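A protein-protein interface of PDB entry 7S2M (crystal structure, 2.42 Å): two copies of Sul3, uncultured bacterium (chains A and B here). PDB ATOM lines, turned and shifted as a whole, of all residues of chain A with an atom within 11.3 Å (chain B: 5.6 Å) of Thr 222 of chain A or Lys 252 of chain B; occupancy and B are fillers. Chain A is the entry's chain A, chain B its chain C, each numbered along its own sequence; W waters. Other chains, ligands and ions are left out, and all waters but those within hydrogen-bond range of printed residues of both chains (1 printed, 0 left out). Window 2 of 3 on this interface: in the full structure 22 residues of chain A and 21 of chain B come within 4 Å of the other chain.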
ATOM      1  N   ARG A 212      20.286  13.959   5.375  1.00  0.00           N
ATOM      2  CA  ARG A 212      19.159  14.577   6.075  1.00  0.00           C
ATOM      3  C   ARG A 212      17.824  13.992   5.609  1.00  0.00           C
ATOM      4  O   ARG A 212      16.974  14.678   5.037  1.00  0.00           O
ATOM      5  CB  ARG A 212      19.183  16.102   5.911  1.00  0.00           C
ATOM      6  CG  ARG A 212      20.576  16.717   5.951  1.00  0.00           C
ATOM      7  CD  ARG A 212      20.650  17.870   6.938  1.00  0.00           C
ATOM      8  NE  ARG A 212      21.899  18.613   6.815  1.00  0.00           N
ATOM      9  CZ  ARG A 212      21.995  19.846   6.339  1.00  0.00           C
ATOM     10  NH1 ARG A 212      20.928  20.516   5.934  1.00  0.00           N
ATOM     11  NH2 ARG A 212      23.191  20.423   6.266  1.00  0.00           N
ATOM     12  N   LYS A 213      17.652  12.699   5.870  1.00  0.00           N
ATOM     13  CA  LYS A 213      16.412  11.998   5.574  1.00  0.00           C
ATOM     14  C   LYS A 213      15.780  11.516   6.873  1.00  0.00           C
ATOM     15  O   LYS A 213      16.476  11.189   7.838  1.00  0.00           O
ATOM     16  CB  LYS A 213      16.649  10.823   4.619  1.00  0.00           C
ATOM     17  CG  LYS A 213      17.388  11.220   3.350  1.00  0.00           C
ATOM     18  CD  LYS A 213      16.563  10.944   2.103  1.00  0.00           C
ATOM     19  CE  LYS A 213      17.228  11.532   0.867  1.00  0.00           C
ATOM     20  NZ  LYS A 213      16.399  11.359  -0.356  1.00  0.00           N
ATOM     21  N   SER A 214      14.444  11.474   6.880  1.00  0.00           N
ATOM     22  CA  SER A 214      13.706  11.260   8.122  1.00  0.00           C
ATOM     23  C   SER A 214      13.956   9.879   8.719  1.00  0.00           C
ATOM     24  O   SER A 214      13.855   9.712   9.940  1.00  0.00           O
ATOM     25  CB  SER A 214      12.210  11.465   7.878  1.00  0.00           C
ATOM     26  OG  SER A 214      11.480  11.414   9.092  1.00  0.00           O
ATOM     27  N   PHE A 215      14.281   8.885   7.888  1.00  0.00           N
ATOM     28  CA  PHE A 215      14.476   7.533   8.406  1.00  0.00           C
ATOM     29  C   PHE A 215      15.684   7.447   9.331  1.00  0.00           C
ATOM     30  O   PHE A 215      15.731   6.574  10.205  1.00  0.00           O
ATOM     31  CB  PHE A 215      14.619   6.542   7.250  1.00  0.00           C
ATOM     32  CG  PHE A 215      16.007   6.461   6.687  1.00  0.00           C
ATOM     33  CD1 PHE A 215      16.456   7.408   5.783  1.00  0.00           C
ATOM     34  CD2 PHE A 215      16.865   5.438   7.061  1.00  0.00           C
ATOM     35  CE1 PHE A 215      17.734   7.339   5.263  1.00  0.00           C
ATOM     36  CE2 PHE A 215      18.144   5.363   6.545  1.00  0.00           C
ATOM     37  CZ  PHE A 215      18.578   6.316   5.645  1.00  0.00           C
ATOM     38  N   LEU A 216      16.666   8.337   9.157  1.00  0.00           N
ATOM     39  CA  LEU A 216      17.830   8.334  10.037  1.00  0.00           C
ATOM     40  C   LEU A 216      17.443   8.696  11.466  1.00  0.00           C
ATOM     41  O   LEU A 216      18.017   8.164  12.425  1.00  0.00           O
ATOM     42  CB  LEU A 216      18.893   9.295   9.506  1.00  0.00           C
ATOM     43  CG  LEU A 216      19.546   8.908   8.176  1.00  0.00           C
ATOM     44  CD1 LEU A 216      20.363  10.061   7.610  1.00  0.00           C
ATOM     45  CD2 LEU A 216      20.411   7.670   8.354  1.00  0.00           C
ATOM     46  N   GLY A 217      16.471   9.596  11.630  1.00  0.00           N
ATOM     47  CA  GLY A 217      16.011   9.943  12.962  1.00  0.00           C
ATOM     48  C   GLY A 217      15.228   8.833  13.629  1.00  0.00           C
ATOM     49  O   GLY A 217      15.239   8.714  14.857  1.00  0.00           O
ATOM     50  N   LYS A 218      14.542   8.007  12.837  1.00  0.00           N
ATOM     51  CA  LYS A 218      13.789   6.892  13.395  1.00  0.00           C
ATOM     52  C   LYS A 218      14.699   5.815  13.967  1.00  0.00           C
ATOM     53  O   LYS A 218      14.250   5.015  14.794  1.00  0.00           O
ATOM     54  CB  LYS A 218      12.872   6.294  12.326  1.00  0.00           C
ATOM     55  CG  LYS A 218      11.933   7.308  11.684  1.00  0.00           C
ATOM     56  CD  LYS A 218      11.301   6.767  10.409  1.00  0.00           C
ATOM     57  CE  LYS A 218      10.058   5.946  10.710  1.00  0.00           C
ATOM     58  NZ  LYS A 218       9.449   6.322  12.015  1.00  0.00           N
ATOM     59  N   ILE A 219      15.963   5.780  13.555  1.00  0.00           N
ATOM     60  CA  ILE A 219      16.901   4.782  14.060  1.00  0.00           C
ATOM     61  C   ILE A 219      17.544   5.236  15.366  1.00  0.00           C
ATOM     62  O   ILE A 219      17.779   4.423  16.264  1.00  0.00           O
ATOM     63  CB  ILE A 219      17.961   4.473  12.984  1.00  0.00           C
ATOM     64  CG1 ILE A 219      17.292   3.920  11.724  1.00  0.00           C
ATOM     65  CG2 ILE A 219      18.987   3.482  13.510  1.00  0.00           C
ATOM     66  CD1 ILE A 219      18.267   3.528  10.637  1.00  0.00           C
ATOM     67  N   THR A 220      17.825   6.531  15.499  1.00  0.00           N
ATOM     68  CA  THR A 220      18.471   7.068  16.691  1.00  0.00           C
ATOM     69  C   THR A 220      17.489   7.745  17.640  1.00  0.00           C
ATOM     70  O   THR A 220      17.419   7.385  18.819  1.00  0.00           O
ATOM     71  CB  THR A 220      19.571   8.062  16.296  1.00  0.00           C
ATOM     72  OG1 THR A 220      19.017   9.379  16.199  1.00  0.00           O
ATOM     73  CG2 THR A 220      20.184   7.676  14.960  1.00  0.00           C
ATOM     74  N   GLY A 221      16.730   8.721  17.150  1.00  0.00           N
ATOM     75  CA  GLY A 221      15.822   9.469  17.997  1.00  0.00           C
ATOM     76  C   GLY A 221      16.262  10.905  18.190  1.00  0.00           C
ATOM     77  O   GLY A 221      16.055  11.490  19.258  1.00  0.00           O
ATOM     78  N   THR A 222      16.876  11.481  17.161  1.00  0.00           N
ATOM     79  CA  THR A 222      17.339  12.859  17.190  1.00  0.00           C
ATOM     80  C   THR A 222      16.885  13.569  15.923  1.00  0.00           C
ATOM     81  O   THR A 222      16.575  12.937  14.910  1.00  0.00           O
ATOM     82  CB  THR A 222      18.866  12.943  17.321  1.00  0.00           C
ATOM     83  OG1 THR A 222      19.471  11.898  16.548  1.00  0.00           O
ATOM     84  CG2 THR A 222      19.287  12.798  18.776  1.00  0.00           C
ATOM     85  N   ASP A 223      16.847  14.896  15.989  1.00  0.00           N
ATOM     86  CA  ASP A 223      16.452  15.709  14.842  1.00  0.00           C
ATOM     87  C   ASP A 223      17.565  15.665  13.803  1.00  0.00           C
ATOM     88  O   ASP A 223      18.574  16.364  13.923  1.00  0.00           O
ATOM     89  CB  ASP A 223      16.156  17.140  15.274  1.00  0.00           C
ATOM     90  CG  ASP A 223      15.682  18.007  14.125  1.00  0.00           C
ATOM     91  OD1 ASP A 223      14.849  17.531  13.324  1.00  0.00           O
ATOM     92  OD2 ASP A 223      16.145  19.162  14.022  1.00  0.00           O
ATOM     93  N   VAL A 224      17.382  14.835  12.772  1.00  0.00           N
ATOM     94  CA  VAL A 224      18.394  14.676  11.731  1.00  0.00           C
ATOM     95  C   VAL A 224      18.261  15.700  10.615  1.00  0.00           C
ATOM     96  O   VAL A 224      19.120  15.739   9.719  1.00  0.00           O
ATOM     97  CB  VAL A 224      18.332  13.261  11.127  1.00  0.00           C
ATOM     98  CG1 VAL A 224      18.523  12.227  12.212  1.00  0.00           C
ATOM     99  CG2 VAL A 224      17.005  13.052  10.416  1.00  0.00           C
ATOM    100  N   LYS A 225      17.214  16.526  10.632  1.00  0.00           N
ATOM    101  CA  LYS A 225      17.027  17.515   9.579  1.00  0.00           C
ATOM    102  C   LYS A 225      18.020  18.666   9.683  1.00  0.00           C
ATOM    103  O   LYS A 225      18.288  19.330   8.676  1.00  0.00           O
ATOM    104  CB  LYS A 225      15.595  18.049   9.615  1.00  0.00           C
ATOM    105  CG  LYS A 225      14.533  16.966   9.489  1.00  0.00           C
ATOM    106  CD  LYS A 225      13.290  17.305  10.299  1.00  0.00           C
ATOM    107  CE  LYS A 225      12.487  18.415   9.639  1.00  0.00           C
ATOM    108  NZ  LYS A 225      11.178  18.640  10.317  1.00  0.00           N
ATOM    109  N   SER A 226      18.572  18.913  10.872  1.00  0.00           N
ATOM    110  CA  SER A 226      19.551  19.974  11.073  1.00  0.00           C
ATOM    111  C   SER A 226      20.858  19.455  11.654  1.00  0.00           C
ATOM    112  O   SER A 226      21.731  20.257  12.008  1.00  0.00           O
ATOM    113  CB  SER A 226      18.977  21.066  11.983  1.00  0.00           C
ATOM    114  OG  SER A 226      17.590  21.247  11.754  1.00  0.00           O
ATOM    115  N   ARG A 227      21.021  18.138  11.759  1.00  0.00           N
ATOM    116  CA  ARG A 227      22.198  17.542  12.368  1.00  0.00           C
ATOM    117  C   ARG A 227      22.926  16.664  11.358  1.00  0.00           C
ATOM    118  O   ARG A 227      22.323  16.132  10.422  1.00  0.00           O
ATOM    119  CB  ARG A 227      21.823  16.721  13.598  1.00  0.00           C
ATOM    120  CG  ARG A 227      21.921  17.484  14.905  1.00  0.00           C
ATOM    121  CD  ARG A 227      21.713  16.529  16.053  1.00  0.00           C
ATOM    122  NE  ARG A 227      22.246  15.222  15.700  1.00  0.00           N
ATOM    123  CZ  ARG A 227      22.655  14.312  16.572  1.00  0.00           C
ATOM    124  NH1 ARG A 227      22.616  14.534  17.872  1.00  0.00           N
ATOM    125  NH2 ARG A 227      23.120  13.149  16.125  1.00  0.00           N
ATOM    126  N   LEU A 228      24.230  16.505  11.574  1.00  0.00           N
ATOM    127  CA  LEU A 228      25.114  15.867  10.609  1.00  0.00           C
ATOM    128  C   LEU A 228      25.592  14.483  11.022  1.00  0.00           C
ATOM    129  O   LEU A 228      25.822  13.643  10.149  1.00  0.00           O
ATOM    130  CB  LEU A 228      26.333  16.763  10.350  1.00  0.00           C
ATOM    131  CG  LEU A 228      27.650  16.110   9.934  1.00  0.00           C
ATOM    132  CD1 LEU A 228      27.742  16.030   8.420  1.00  0.00           C
ATOM    133  CD2 LEU A 228      28.831  16.872  10.517  1.00  0.00           C
ATOM    134  N   ALA A 229      25.728  14.221  12.323  1.00  0.00           N
ATOM    135  CA  ALA A 229      26.282  12.953  12.799  1.00  0.00           C
ATOM    136  C   ALA A 229      25.606  11.717  12.214  1.00  0.00           C
ATOM    137  O   ALA A 229      26.323  10.828  11.729  1.00  0.00           O
ATOM    138  CB  ALA A 229      26.237  12.929  14.333  1.00  0.00           C
ATOM    139  N   PRO A 230      24.274  11.580  12.220  1.00  0.00           N
ATOM    140  CA  PRO A 230      23.684  10.391  11.587  1.00  0.00           C
ATOM    141  C   PRO A 230      23.775  10.421  10.073  1.00  0.00           C
ATOM    142  O   PRO A 230      23.889   9.358   9.450  1.00  0.00           O
ATOM    143  CB  PRO A 230      22.230  10.422  12.072  1.00  0.00           C
ATOM    144  CG  PRO A 230      21.957  11.858  12.275  1.00  0.00           C
ATOM    145  CD  PRO A 230      23.233  12.464  12.782  1.00  0.00           C
ATOM    146  N   THR A 231      23.724  11.607   9.463  1.00  0.00           N
ATOM    147  CA  THR A 231      23.936  11.709   8.023  1.00  0.00           C
ATOM    148  C   THR A 231      25.346  11.273   7.648  1.00  0.00           C
ATOM    149  O   THR A 231      25.545  10.572   6.648  1.00  0.00           O
ATOM    150  CB  THR A 231      23.668  13.143   7.559  1.00  0.00           C
ATOM    151  OG1 THR A 231      22.254  13.378   7.517  1.00  0.00           O
ATOM    152  CG2 THR A 231      24.255  13.388   6.178  1.00  0.00           C
ATOM    153  N   LEU A 232      26.340  11.662   8.451  1.00  0.00           N
ATOM    154  CA  LEU A 232      27.721  11.293   8.158  1.00  0.00           C
ATOM    155  C   LEU A 232      27.956   9.803   8.365  1.00  0.00           C
ATOM    156  O   LEU A 232      28.692   9.174   7.596  1.00  0.00           O
ATOM    157  CB  LEU A 232      28.677  12.107   9.029  1.00  0.00           C
ATOM    158  CG  LEU A 232      30.077  12.334   8.458  1.00  0.00           C
ATOM    159  CD1 LEU A 232      30.030  13.297   7.282  1.00  0.00           C
ATOM    160  CD2 LEU A 232      31.018  12.836   9.538  1.00  0.00           C
ATOM    161  N   ALA A 233      27.351   9.224   9.406  1.00  0.00           N
ATOM    162  CA  ALA A 233      27.537   7.801   9.666  1.00  0.00           C
ATOM    163  C   ALA A 233      27.013   6.956   8.513  1.00  0.00           C
ATOM    164  O   ALA A 233      27.650   5.975   8.112  1.00  0.00           O
ATOM    165  CB  ALA A 233      26.851   7.411  10.976  1.00  0.00           C
ATOM    166  N   LEU B  36      24.797  14.689  28.983  1.00  0.00           N
ATOM    167  CA  LEU B  36      25.544  13.676  28.246  1.00  0.00           C
ATOM    168  C   LEU B  36      24.997  12.282  28.524  1.00  0.00           C
ATOM    169  O   LEU B  36      24.938  11.439  27.620  1.00  0.00           O
ATOM    170  CB  LEU B  36      27.029  13.754  28.601  1.00  0.00           C
ATOM    171  CG  LEU B  36      27.778  14.988  28.094  1.00  0.00           C
ATOM    172  CD1 LEU B  36      29.229  14.955  28.542  1.00  0.00           C
ATOM    173  CD2 LEU B  36      27.681  15.101  26.580  1.00  0.00           C
ATOM    174  N   ASP B  39      22.216  11.676  26.544  1.00  0.00           N
ATOM    175  CA  ASP B  39      22.586  11.623  25.139  1.00  0.00           C
ATOM    176  C   ASP B  39      23.155  10.277  24.712  1.00  0.00           C
ATOM    177  O   ASP B  39      23.386  10.076  23.514  1.00  0.00           O
ATOM    178  CB  ASP B  39      23.603  12.727  24.817  1.00  0.00           C
ATOM    179  CG  ASP B  39      22.942  14.068  24.573  1.00  0.00           C
ATOM    180  OD1 ASP B  39      21.695  14.120  24.570  1.00  0.00           O
ATOM    181  OD2 ASP B  39      23.668  15.067  24.379  1.00  0.00           O
ATOM    182  N   ASP B 250      31.555  15.416  22.042  1.00  0.00           N
ATOM    183  CA  ASP B 250      30.215  15.305  21.470  1.00  0.00           C
ATOM    184  C   ASP B 250      29.744  13.863  21.609  1.00  0.00           C
ATOM    185  O   ASP B 250      30.133  12.989  20.831  1.00  0.00           O
ATOM    186  CB  ASP B 250      30.220  15.747  20.011  1.00  0.00           C
ATOM    187  CG  ASP B 250      28.921  16.412  19.599  1.00  0.00           C
ATOM    188  OD1 ASP B 250      27.846  15.932  20.019  1.00  0.00           O
ATOM    189  OD2 ASP B 250      28.973  17.412  18.852  1.00  0.00           O
ATOM    190  N   VAL B 251      28.903  13.607  22.606  1.00  0.00           N
ATOM    191  CA  VAL B 251      28.438  12.252  22.887  1.00  0.00           C
ATOM    192  C   VAL B 251      27.222  11.895  22.044  1.00  0.00           C
ATOM    193  O   VAL B 251      27.152  10.806  21.468  1.00  0.00           O
ATOM    194  CB  VAL B 251      28.142  12.101  24.395  1.00  0.00           C
ATOM    195  CG1 VAL B 251      27.335  10.839  24.655  1.00  0.00           C
ATOM    196  CG2 VAL B 251      29.438  12.089  25.190  1.00  0.00           C
ATOM    197  N   LYS B 252      26.247  12.806  21.956  1.00  0.00           N
ATOM    198  CA  LYS B 252      25.054  12.536  21.157  1.00  0.00           C
ATOM    199  C   LYS B 252      25.395  12.351  19.686  1.00  0.00           C
ATOM    200  O   LYS B 252      24.694  11.624  18.974  1.00  0.00           O
ATOM    201  CB  LYS B 252      24.030  13.660  21.343  1.00  0.00           C
ATOM    202  CG  LYS B 252      22.583  13.247  21.088  1.00  0.00           C
ATOM    203  CD  LYS B 252      21.593  14.374  21.417  1.00  0.00           C
ATOM    204  CE  LYS B 252      21.934  15.691  20.731  1.00  0.00           C
ATOM    205  NZ  LYS B 252      21.537  16.886  21.529  1.00  0.00           N
ATOM    206  N   SER B 253      26.473  12.981  19.214  1.00  0.00           N
ATOM    207  CA  SER B 253      26.913  12.752  17.842  1.00  0.00           C
ATOM    208  C   SER B 253      27.500  11.355  17.675  1.00  0.00           C
ATOM    209  O   SER B 253      27.224  10.675  16.680  1.00  0.00           O
ATOM    210  CB  SER B 253      27.928  13.819  17.433  1.00  0.00           C
ATOM    211  OG  SER B 253      27.300  15.076  17.261  1.00  0.00           O
ATOM    212  N   LEU B 254      28.309  10.910  18.639  1.00  0.00           N
ATOM    213  CA  LEU B 254      28.867   9.563  18.569  1.00  0.00           C
ATOM    214  C   LEU B 254      27.798   8.510  18.830  1.00  0.00           C
ATOM    215  O   LEU B 254      27.797   7.447  18.196  1.00  0.00           O
ATOM    216  CB  LEU B 254      30.017   9.414  19.564  1.00  0.00           C
ATOM    217  CG  LEU B 254      30.604   8.008  19.702  1.00  0.00           C
ATOM    218  CD1 LEU B 254      31.228   7.557  18.388  1.00  0.00           C
ATOM    219  CD2 LEU B 254      31.618   7.950  20.831  1.00  0.00           C
ATOM    220  N   SER B 255      26.881   8.785  19.762  1.00  0.00           N
ATOM    221  CA  SER B 255      25.818   7.831  20.063  1.00  0.00           C
ATOM    222  C   SER B 255      24.955   7.561  18.839  1.00  0.00           C
ATOM    223  O   SER B 255      24.551   6.419  18.596  1.00  0.00           O
ATOM    224  CB  SER B 255      24.961   8.343  21.219  1.00  0.00           C
ATOM    225  OG  SER B 255      24.273   7.277  21.851  1.00  0.00           O
ATOM    226  N   ASP B 256      24.659   8.601  18.058  1.00  0.00           N
ATOM    227  CA  ASP B 256      23.893   8.409  16.833  1.00  0.00           C
ATOM    228  C   ASP B 256      24.743   7.820  15.716  1.00  0.00           C
ATOM    229  O   ASP B 256      24.220   7.087  14.869  1.00  0.00           O
ATOM    230  CB  ASP B 256      23.270   9.731  16.384  1.00  0.00           C
ATOM    231  CG  ASP B 256      22.373  10.340  17.444  1.00  0.00           C
ATOM    232  OD1 ASP B 256      22.079   9.652  18.443  1.00  0.00           O
ATOM    233  OD2 ASP B 256      21.955  11.503  17.272  1.00  0.00           O
ATOM    234  N   ALA B 257      26.042   8.124  15.692  1.00  0.00           N
ATOM    235  CA  ALA B 257      26.917   7.487  14.714  1.00  0.00           C
ATOM    236  C   ALA B 257      27.040   5.993  14.984  1.00  0.00           C
ATOM    237  O   ALA B 257      27.137   5.192  14.047  1.00  0.00           O
ATOM    238  CB  ALA B 257      28.294   8.150  14.723  1.00  0.00           C
HETATM  239  O   HOH W   1      25.792  16.069  15.216  1.00  0.00           O
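The side-chain carboxylate (OD2) of Asp 256 of chain B lies within hydrogen-bond range of the side-chain hydroxyl (OG1) of Thr 222 of chain A, at 2.6 Å.
The side-chain carboxylate (OD2) of Asp 256 of chain B is in salt-bridge range of the guanidinium group (NH1) of Arg 227 of chain A (3.2 Å).
The side-chain hydroxyl (OG1) of Thr 220 of chain A lies within hydrogen-bond range of the side-chain hydroxyl (OG1) of Thr 222 of chain A.
OD2 of Asp 39 of chain B lies within salt-bridge range of NZ of Lys 252 of chain B, 3.997 Å away.
OD1 of Asp 250 of chain B sits at hydrogen-bond distance from OG of Ser 253 of chain B, at 2.9 Å.
Among the printed residues, merely in contact across the chains: Arg 227 of chain A with Lys 252 of chain B, Ala 229 of chain A with Ser 253 of chain B, Thr 220 of chain A with Asp 256 of chain B, Ala 233 of chain A with Ala 257 of chain B and Thr 222 of chain A with Lys 252 of chain B.
Of chain B, only Lys 252 (3.8 Å) and Asp 256 (2.6 Å) come within 4 Å of Thr 222 of chain A.
Printed residues of chain A within 4 Å of Lys 252 of chain B: Thr 222 and Arg 227.
No residue of chain A comes within 4 Å of Asp 39 of chain B.
No residue of chain A comes within 4 Å of Asp 250 of chain B.
No residue of chain A comes within 4 Å of Val 251 of chain B.
Asp 256 of chain B touches just these residues of chain A: Thr 220, Thr 222 and Arg 227.
Printed residues of chain B within 4 Å of Ala 229 of chain A: Ser 253.
Printed residues of chain B within 4 Å of Arg 227 of chain A: Lys 252 (3.2 Å) and Asp 256 (2.3 Å).
Printed residues of chain A within 4 Å of Ala 257 of chain B: Ala 233 (3.7 Å).
Of the printed residues of chain B, Thr 220 of chain A touches Asp 256 (3.7 Å).
Ser 214 of chain A touches none of the printed residues of chain B.
The nearest residue of chain A that does not touch Lys 252 of chain B is Ala 229 of chain A (5.1 Å).
The nearest printed residue of chain B that does not touch Arg 227 of chain A is Ser 253 of chain B (4.2 Å).
Printed residues of chain A that touch a printed residue of chain B: Thr 220, Thr 222, Arg 227, Ala 229 and Ala 233.
Hydrophobic or aromatic side chains of chain A that line the printed part of chain B: Ala 229 and Ala 233.
Of the 10 printed residues of chain B, 4 touch a printed residue of chain A.
Among the printed residues, 7 pairs touch across the chains.
Among the printed residues, Asp or Glu carboxylates within 4 Å of a Lys or Arg side-chain nitrogen of the other chain: Arg 227 of chain A with Asp 256 of chain B.
No position is printed for both chains.
Water W1 bridges the side-chain hydroxyl (OG) of Ser 253 of chain B (2.7 Å) and the backbone NH (N) of Ala 229 of chain A (3.4 Å).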
